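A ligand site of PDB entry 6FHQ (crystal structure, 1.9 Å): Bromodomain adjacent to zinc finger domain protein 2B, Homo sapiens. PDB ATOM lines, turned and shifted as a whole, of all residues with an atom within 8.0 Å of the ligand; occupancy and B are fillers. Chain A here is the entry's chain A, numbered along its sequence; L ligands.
The backbone NH of Leu 23 sits at hydrogen-bond distance from an oxygen (O1) of the ligand (2.9 Å).
O of Leu 23 lies within hydrogen-bond range of N3 of the ligand, at 2.6 Å.
A nitrogen (N3) of the ligand lies within salt-bridge range of the side-chain carboxylate (OD2) of Asp 25, 2.8 Å away.
The backbone carbonyl oxygen of Trp 48 sits at hydrogen-bond distance from the backbone NH of Asp 25 (2.8 Å).
N of Leu 22 sits at hydrogen-bond distance from O of Cys 31.
S1 of the ligand sits close to O of Leu 21, at 3.4 Å.
Glu 18 touches the ligand.
Glu 19 touches the ligand (O to C5, 3.2 Å).
Leu 22 touches the ligand.
Ile 43 touches the ligand.
Pro 44 touches the ligand (O to N1, 3.98 Å).
Gly 46 touches the ligand.
Asp 47 touches the ligand.
Trp 48 touches the ligand (N to C2, 3.7 Å).
Within 4 Å of the ligand: Glu 18, Glu 19, Leu 21, Leu 22, Leu 23, Asp 25, Ile 43, Pro 44, Gly 46, Asp 47 and Trp 48.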
ATOM      1  N   ASN A  17     -36.562  37.283 -29.534  1.00  0.00           N
ATOM      2  CA  ASN A  17     -36.109  36.219 -30.421  1.00  0.00           C
ATOM      3  C   ASN A  17     -35.629  35.066 -29.611  1.00  0.00           C
ATOM      4  O   ASN A  17     -34.503  34.643 -29.724  1.00  0.00           O
ATOM      5  CB  ASN A  17     -34.945  36.690 -31.266  1.00  0.00           C
ATOM      6  CG  ASN A  17     -35.368  37.215 -32.598  1.00  0.00           C
ATOM      7  OD1 ASN A  17     -36.225  36.639 -33.268  1.00  0.00           O
ATOM      8  ND2 ASN A  17     -34.726  38.267 -33.020  1.00  0.00           N
ATOM      9  N   GLU A  18     -36.516  34.568 -28.778  1.00  0.00           N
ATOM     10  CA  GLU A  18     -36.189  33.555 -27.820  1.00  0.00           C
ATOM     11  C   GLU A  18     -35.761  32.209 -28.414  1.00  0.00           C
ATOM     12  O   GLU A  18     -35.018  31.472 -27.782  1.00  0.00           O
ATOM     13  CB  GLU A  18     -37.425  33.356 -26.898  1.00  0.00           C
ATOM     14  CG  GLU A  18     -37.615  34.584 -25.985  1.00  0.00           C
ATOM     15  CD  GLU A  18     -39.076  35.062 -25.875  1.00  0.00           C
ATOM     16  OE1 GLU A  18     -39.994  34.354 -26.348  1.00  0.00           O
ATOM     17  OE2 GLU A  18     -39.301  36.155 -25.295  1.00  0.00           O
ATOM     18  N   GLU A  19     -36.235  31.926 -29.617  1.00  0.00           N
ATOM     19  CA  GLU A  19     -35.826  30.784 -30.449  1.00  0.00           C
ATOM     20  C   GLU A  19     -34.333  30.834 -30.871  1.00  0.00           C
ATOM     21  O   GLU A  19     -33.782  29.857 -31.394  1.00  0.00           O
ATOM     22  CB  GLU A  19     -36.721  30.760 -31.700  1.00  0.00           C
ATOM     23  CG  GLU A  19     -36.248  29.879 -32.853  1.00  0.00           C
ATOM     24  CD  GLU A  19     -37.395  29.114 -33.492  1.00  0.00           C
ATOM     25  OE1 GLU A  19     -37.864  28.125 -32.879  1.00  0.00           O
ATOM     26  OE2 GLU A  19     -37.812  29.505 -34.613  1.00  0.00           O
ATOM     27  N   LEU A  20     -33.713  31.992 -30.716  1.00  0.00           N
ATOM     28  CA  LEU A  20     -32.371  32.178 -31.172  1.00  0.00           C
ATOM     29  C   LEU A  20     -31.493  32.556 -29.999  1.00  0.00           C
ATOM     30  O   LEU A  20     -30.306  32.785 -30.162  1.00  0.00           O
ATOM     31  CB  LEU A  20     -32.348  33.247 -32.247  1.00  0.00           C
ATOM     32  CG  LEU A  20     -33.070  32.904 -33.538  1.00  0.00           C
ATOM     33  CD1 LEU A  20     -33.039  34.114 -34.453  1.00  0.00           C
ATOM     34  CD2 LEU A  20     -32.429  31.681 -34.216  1.00  0.00           C
ATOM     35  N   LEU A  21     -32.104  32.610 -28.828  1.00  0.00           N
ATOM     36  CA  LEU A  21     -31.425  33.070 -27.674  1.00  0.00           C
ATOM     37  C   LEU A  21     -30.879  31.804 -26.935  1.00  0.00           C
ATOM     38  O   LEU A  21     -31.625  31.087 -26.241  1.00  0.00           O
ATOM     39  CB  LEU A  21     -32.378  33.892 -26.828  1.00  0.00           C
ATOM     40  CG  LEU A  21     -31.841  34.371 -25.492  1.00  0.00           C
ATOM     41  CD1 LEU A  21     -30.579  35.207 -25.636  1.00  0.00           C
ATOM     42  CD2 LEU A  21     -32.960  35.112 -24.704  1.00  0.00           C
ATOM     43  N   LEU A  22     -29.588  31.540 -27.107  1.00  0.00           N
ATOM     44  CA  LEU A  22     -29.063  30.262 -26.695  1.00  0.00           C
ATOM     45  C   LEU A  22     -28.771  30.385 -25.237  1.00  0.00           C
ATOM     46  O   LEU A  22     -28.108  31.325 -24.866  1.00  0.00           O
ATOM     47  CB  LEU A  22     -27.765  29.914 -27.416  1.00  0.00           C
ATOM     48  CG  LEU A  22     -27.782  29.919 -28.912  1.00  0.00           C
ATOM     49  CD1 LEU A  22     -26.418  29.484 -29.447  1.00  0.00           C
ATOM     50  CD2 LEU A  22     -28.905  29.050 -29.450  1.00  0.00           C
ATOM     51  N   LEU A  23     -29.149  29.392 -24.471  1.00  0.00           N
ATOM     52  CA  LEU A  23     -28.990  29.411 -23.013  1.00  0.00           C
ATOM     53  C   LEU A  23     -27.975  28.438 -22.624  1.00  0.00           C
ATOM     54  O   LEU A  23     -28.136  27.238 -22.924  1.00  0.00           O
ATOM     55  CB  LEU A  23     -30.296  29.009 -22.361  1.00  0.00           C
ATOM     56  CG  LEU A  23     -31.484  29.892 -22.738  1.00  0.00           C
ATOM     57  CD1 LEU A  23     -32.691  29.417 -21.887  1.00  0.00           C
ATOM     58  CD2 LEU A  23     -31.140  31.351 -22.449  1.00  0.00           C
ATOM     59  N   CYS A  24     -26.926  28.900 -21.977  1.00  0.00           N
ATOM     60  CA  CYS A  24     -25.844  28.000 -21.624  1.00  0.00           C
ATOM     61  C   CYS A  24     -26.270  27.063 -20.475  1.00  0.00           C
ATOM     62  O   CYS A  24     -26.695  27.530 -19.397  1.00  0.00           O
ATOM     63  CB  CYS A  24     -24.613  28.761 -21.273  1.00  0.00           C
ATOM     64  SG  CYS A  24     -23.225  27.716 -20.729  1.00  0.00           S
ATOM     65  N   ASP A  25     -26.177  25.766 -20.726  1.00  0.00           N
ATOM     66  CA  ASP A  25     -26.496  24.770 -19.686  1.00  0.00           C
ATOM     67  C   ASP A  25     -25.432  24.770 -18.618  1.00  0.00           C
ATOM     68  O   ASP A  25     -25.628  24.209 -17.532  1.00  0.00           O
ATOM     69  CB  ASP A  25     -26.589  23.375 -20.298  1.00  0.00           C
ATOM     70  CG  ASP A  25     -27.844  23.206 -21.118  1.00  0.00           C
ATOM     71  OD1 ASP A  25     -28.921  23.082 -20.523  1.00  0.00           O
ATOM     72  OD2 ASP A  25     -27.764  23.315 -22.363  1.00  0.00           O
ATOM     73  N   GLY A  26     -24.280  25.399 -18.907  1.00  0.00           N
ATOM     74  CA  GLY A  26     -23.216  25.569 -17.936  1.00  0.00           C
ATOM     75  C   GLY A  26     -23.493  26.623 -16.904  1.00  0.00           C
ATOM     76  O   GLY A  26     -23.449  26.334 -15.712  1.00  0.00           O
ATOM     77  N   ASP A  28     -25.930  29.206 -17.250  1.00  0.00           N
ATOM     78  CA  ASP A  28     -27.238  29.834 -17.495  1.00  0.00           C
ATOM     79  C   ASP A  28     -27.324  31.250 -18.118  1.00  0.00           C
ATOM     80  O   ASP A  28     -28.427  31.803 -18.208  1.00  0.00           O
ATOM     81  CB  ASP A  28     -28.094  29.754 -16.211  1.00  0.00           C
ATOM     82  CG  ASP A  28     -28.243  28.345 -15.734  1.00  0.00           C
ATOM     83  OD1 ASP A  28     -28.878  27.546 -16.454  1.00  0.00           O
ATOM     84  OD2 ASP A  28     -27.560  27.994 -14.757  1.00  0.00           O
ATOM     85  N   LYS A  29     -26.238  31.786 -18.655  1.00  0.00           N
ATOM     86  CA  LYS A  29     -26.301  33.066 -19.370  1.00  0.00           C
ATOM     87  C   LYS A  29     -26.861  32.845 -20.791  1.00  0.00           C
ATOM     88  O   LYS A  29     -26.848  31.736 -21.275  1.00  0.00           O
ATOM     89  CB  LYS A  29     -24.944  33.671 -19.416  1.00  0.00           C
ATOM     90  CG  LYS A  29     -24.463  34.056 -18.016  1.00  0.00           C
ATOM     91  CD  LYS A  29     -23.246  34.942 -18.098  1.00  0.00           C
ATOM     92  CE  LYS A  29     -23.061  35.757 -16.793  1.00  0.00           C
ATOM     93  NZ  LYS A  29     -21.628  36.196 -16.689  1.00  0.00           N
ATOM     94  N   GLY A  30     -27.345  33.920 -21.432  1.00  0.00           N
ATOM     95  CA  GLY A  30     -27.889  33.856 -22.785  1.00  0.00           C
ATOM     96  C   GLY A  30     -27.150  34.685 -23.800  1.00  0.00           C
ATOM     97  O   GLY A  30     -26.488  35.658 -23.484  1.00  0.00           O
ATOM     98  N   CYS A  31     -27.203  34.248 -25.060  1.00  0.00           N
ATOM     99  CA  CYS A  31     -26.665  35.032 -26.142  1.00  0.00           C
ATOM    100  C   CYS A  31     -27.311  34.607 -27.421  1.00  0.00           C
ATOM    101  O   CYS A  31     -27.457  33.406 -27.680  1.00  0.00           O
ATOM    102  CB  CYS A  31     -25.156  34.849 -26.208  1.00  0.00           C
ATOM    103  SG  CYS A  31     -24.277  35.953 -27.334  1.00  0.00           S
ATOM    104  N   THR A  33     -27.831  33.729 -31.309  1.00  0.00           N
ATOM    105  CA  THR A  33     -26.998  33.206 -32.383  1.00  0.00           C
ATOM    106  C   THR A  33     -26.259  34.318 -33.161  1.00  0.00           C
ATOM    107  O   THR A  33     -25.026  34.278 -33.368  1.00  0.00           O
ATOM    108  CB  THR A  33     -27.855  32.459 -33.418  1.00  0.00           C
ATOM    109  OG1 THR A  33     -29.034  33.214 -33.704  1.00  0.00           O
ATOM    110  CG2 THR A  33     -28.243  31.116 -32.927  1.00  0.00           C
ATOM    111  N   THR A  42     -25.880  27.570 -36.898  1.00  0.00           N
ATOM    112  CA  THR A  42     -26.645  26.315 -36.622  1.00  0.00           C
ATOM    113  C   THR A  42     -27.347  26.431 -35.291  1.00  0.00           C
ATOM    114  O   THR A  42     -26.676  26.562 -34.302  1.00  0.00           O
ATOM    115  CB  THR A  42     -25.703  25.069 -36.562  1.00  0.00           C
ATOM    116  OG1 THR A  42     -25.156  24.819 -37.867  1.00  0.00           O
ATOM    117  CG2 THR A  42     -26.474  23.802 -36.109  1.00  0.00           C
ATOM    118  N   ILE A  43     -28.670  26.287 -35.241  1.00  0.00           N
ATOM    119  CA  ILE A  43     -29.358  26.207 -33.924  1.00  0.00           C
ATOM    120  C   ILE A  43     -29.066  24.857 -33.221  1.00  0.00           C
ATOM    121  O   ILE A  43     -29.275  23.773 -33.818  1.00  0.00           O
ATOM    122  CB  ILE A  43     -30.879  26.453 -33.998  1.00  0.00           C
ATOM    123  CG1 ILE A  43     -31.172  27.892 -34.445  1.00  0.00           C
ATOM    124  CG2 ILE A  43     -31.543  26.280 -32.627  1.00  0.00           C
ATOM    125  CD1 ILE A  43     -32.488  28.023 -35.210  1.00  0.00           C
ATOM    126  N   PRO A  44     -28.529  24.904 -31.989  1.00  0.00           N
ATOM    127  CA  PRO A  44     -28.057  23.656 -31.400  1.00  0.00           C
ATOM    128  C   PRO A  44     -29.242  22.742 -31.235  1.00  0.00           C
ATOM    129  O   PRO A  44     -30.316  23.194 -30.849  1.00  0.00           O
ATOM    130  CB  PRO A  44     -27.498  24.067 -30.008  1.00  0.00           C
ATOM    131  CG  PRO A  44     -27.075  25.495 -30.212  1.00  0.00           C
ATOM    132  CD  PRO A  44     -28.060  26.083 -31.212  1.00  0.00           C
ATOM    133  N   ASP A  45     -29.079  21.479 -31.615  1.00  0.00           N
ATOM    134  CA  ASP A  45     -30.168  20.551 -31.510  1.00  0.00           C
ATOM    135  C   ASP A  45     -30.402  20.030 -30.080  1.00  0.00           C
ATOM    136  O   ASP A  45     -31.511  19.643 -29.747  1.00  0.00           O
ATOM    137  CB  ASP A  45     -29.911  19.368 -32.469  1.00  0.00           C
ATOM    138  CG  ASP A  45     -31.131  18.538 -32.655  1.00  0.00           C
ATOM    139  OD1 ASP A  45     -32.243  19.170 -32.709  1.00  0.00           O
ATOM    140  OD2 ASP A  45     -30.990  17.282 -32.626  1.00  0.00           O
ATOM    141  N   GLY A  46     -29.369  20.080 -29.231  1.00  0.00           N
ATOM    142  CA  GLY A  46     -29.448  19.582 -27.871  1.00  0.00           C
ATOM    143  C   GLY A  46     -29.084  20.680 -26.867  1.00  0.00           C
ATOM    144  O   GLY A  46     -29.677  21.761 -26.819  1.00  0.00           O
ATOM    145  N   ASP A  47     -28.068  20.419 -26.103  1.00  0.00           N
ATOM    146  CA  ASP A  47     -27.638  21.435 -25.151  1.00  0.00           C
ATOM    147  C   ASP A  47     -26.527  22.300 -25.686  1.00  0.00           C
ATOM    148  O   ASP A  47     -25.906  21.974 -26.658  1.00  0.00           O
ATOM    149  CB  ASP A  47     -27.272  20.795 -23.865  1.00  0.00           C
ATOM    150  CG  ASP A  47     -28.495  20.209 -23.142  1.00  0.00           C
ATOM    151  OD1 ASP A  47     -29.626  20.859 -23.007  1.00  0.00           O
ATOM    152  OD2 ASP A  47     -28.286  19.120 -22.625  1.00  0.00           O
ATOM    153  N   TRP A  48     -26.407  23.462 -25.076  1.00  0.00           N
ATOM    154  CA  TRP A  48     -25.491  24.535 -25.473  1.00  0.00           C
ATOM    155  C   TRP A  48     -24.593  24.868 -24.286  1.00  0.00           C
ATOM    156  O   TRP A  48     -25.088  25.029 -23.191  1.00  0.00           O
ATOM    157  CB  TRP A  48     -26.288  25.783 -25.777  1.00  0.00           C
ATOM    158  CG  TRP A  48     -25.453  26.941 -26.122  1.00  0.00           C
ATOM    159  CD1 TRP A  48     -25.344  28.109 -25.426  1.00  0.00           C
ATOM    160  CD2 TRP A  48     -24.542  27.004 -27.168  1.00  0.00           C
ATOM    161  NE1 TRP A  48     -24.453  28.906 -26.017  1.00  0.00           N
ATOM    162  CE2 TRP A  48     -23.898  28.246 -27.081  1.00  0.00           C
ATOM    163  CE3 TRP A  48     -24.148  26.106 -28.155  1.00  0.00           C
ATOM    164  CZ2 TRP A  48     -22.973  28.670 -27.997  1.00  0.00           C
ATOM    165  CZ3 TRP A  48     -23.197  26.515 -29.058  1.00  0.00           C
ATOM    166  CH2 TRP A  48     -22.617  27.795 -28.988  1.00  0.00           C
ATOM    167  N   PHE A  49     -23.288  24.896 -24.516  1.00  0.00           N
ATOM    168  CA  PHE A  49     -22.335  25.473 -23.599  1.00  0.00           C
ATOM    169  C   PHE A  49     -21.649  26.656 -24.269  1.00  0.00           C
ATOM    170  O   PHE A  49     -21.149  26.556 -25.421  1.00  0.00           O
ATOM    171  CB  PHE A  49     -21.336  24.422 -23.180  1.00  0.00           C
ATOM    172  CG  PHE A  49     -21.953  23.332 -22.359  1.00  0.00           C
ATOM    173  CD1 PHE A  49     -22.221  23.527 -21.003  1.00  0.00           C
ATOM    174  CD2 PHE A  49     -22.351  22.127 -22.974  1.00  0.00           C
ATOM    175  CE1 PHE A  49     -22.882  22.539 -20.280  1.00  0.00           C
ATOM    176  CE2 PHE A  49     -22.983  21.134 -22.210  1.00  0.00           C
ATOM    177  CZ  PHE A  49     -23.255  21.348 -20.903  1.00  0.00           C
HETATM  178  C1  LIG L   1     -30.544  25.894 -25.745  1.00  0.00           C
HETATM  179  C2  LIG L   1     -29.866  24.723 -24.950  1.00  0.00           C
HETATM  180  N1  LIG L   1     -32.264  26.081 -28.915  1.00  0.00           N
HETATM  181  N2  LIG L   1     -31.155  25.480 -26.903  1.00  0.00           N
HETATM  182  C3  LIG L   1     -31.835  26.355 -27.682  1.00  0.00           C
HETATM  183  N3  LIG L   1     -29.522  25.082 -23.535  1.00  0.00           N
HETATM  184  C4  LIG L   1     -32.935  27.097 -29.533  1.00  0.00           C
HETATM  185  C5  LIG L   1     -33.032  28.215 -28.783  1.00  0.00           C
HETATM  186  S1  LIG L   1     -32.307  27.945 -27.293  1.00  0.00           S
HETATM  187  O1  LIG L   1     -30.580  27.066 -25.292  1.00  0.00           O
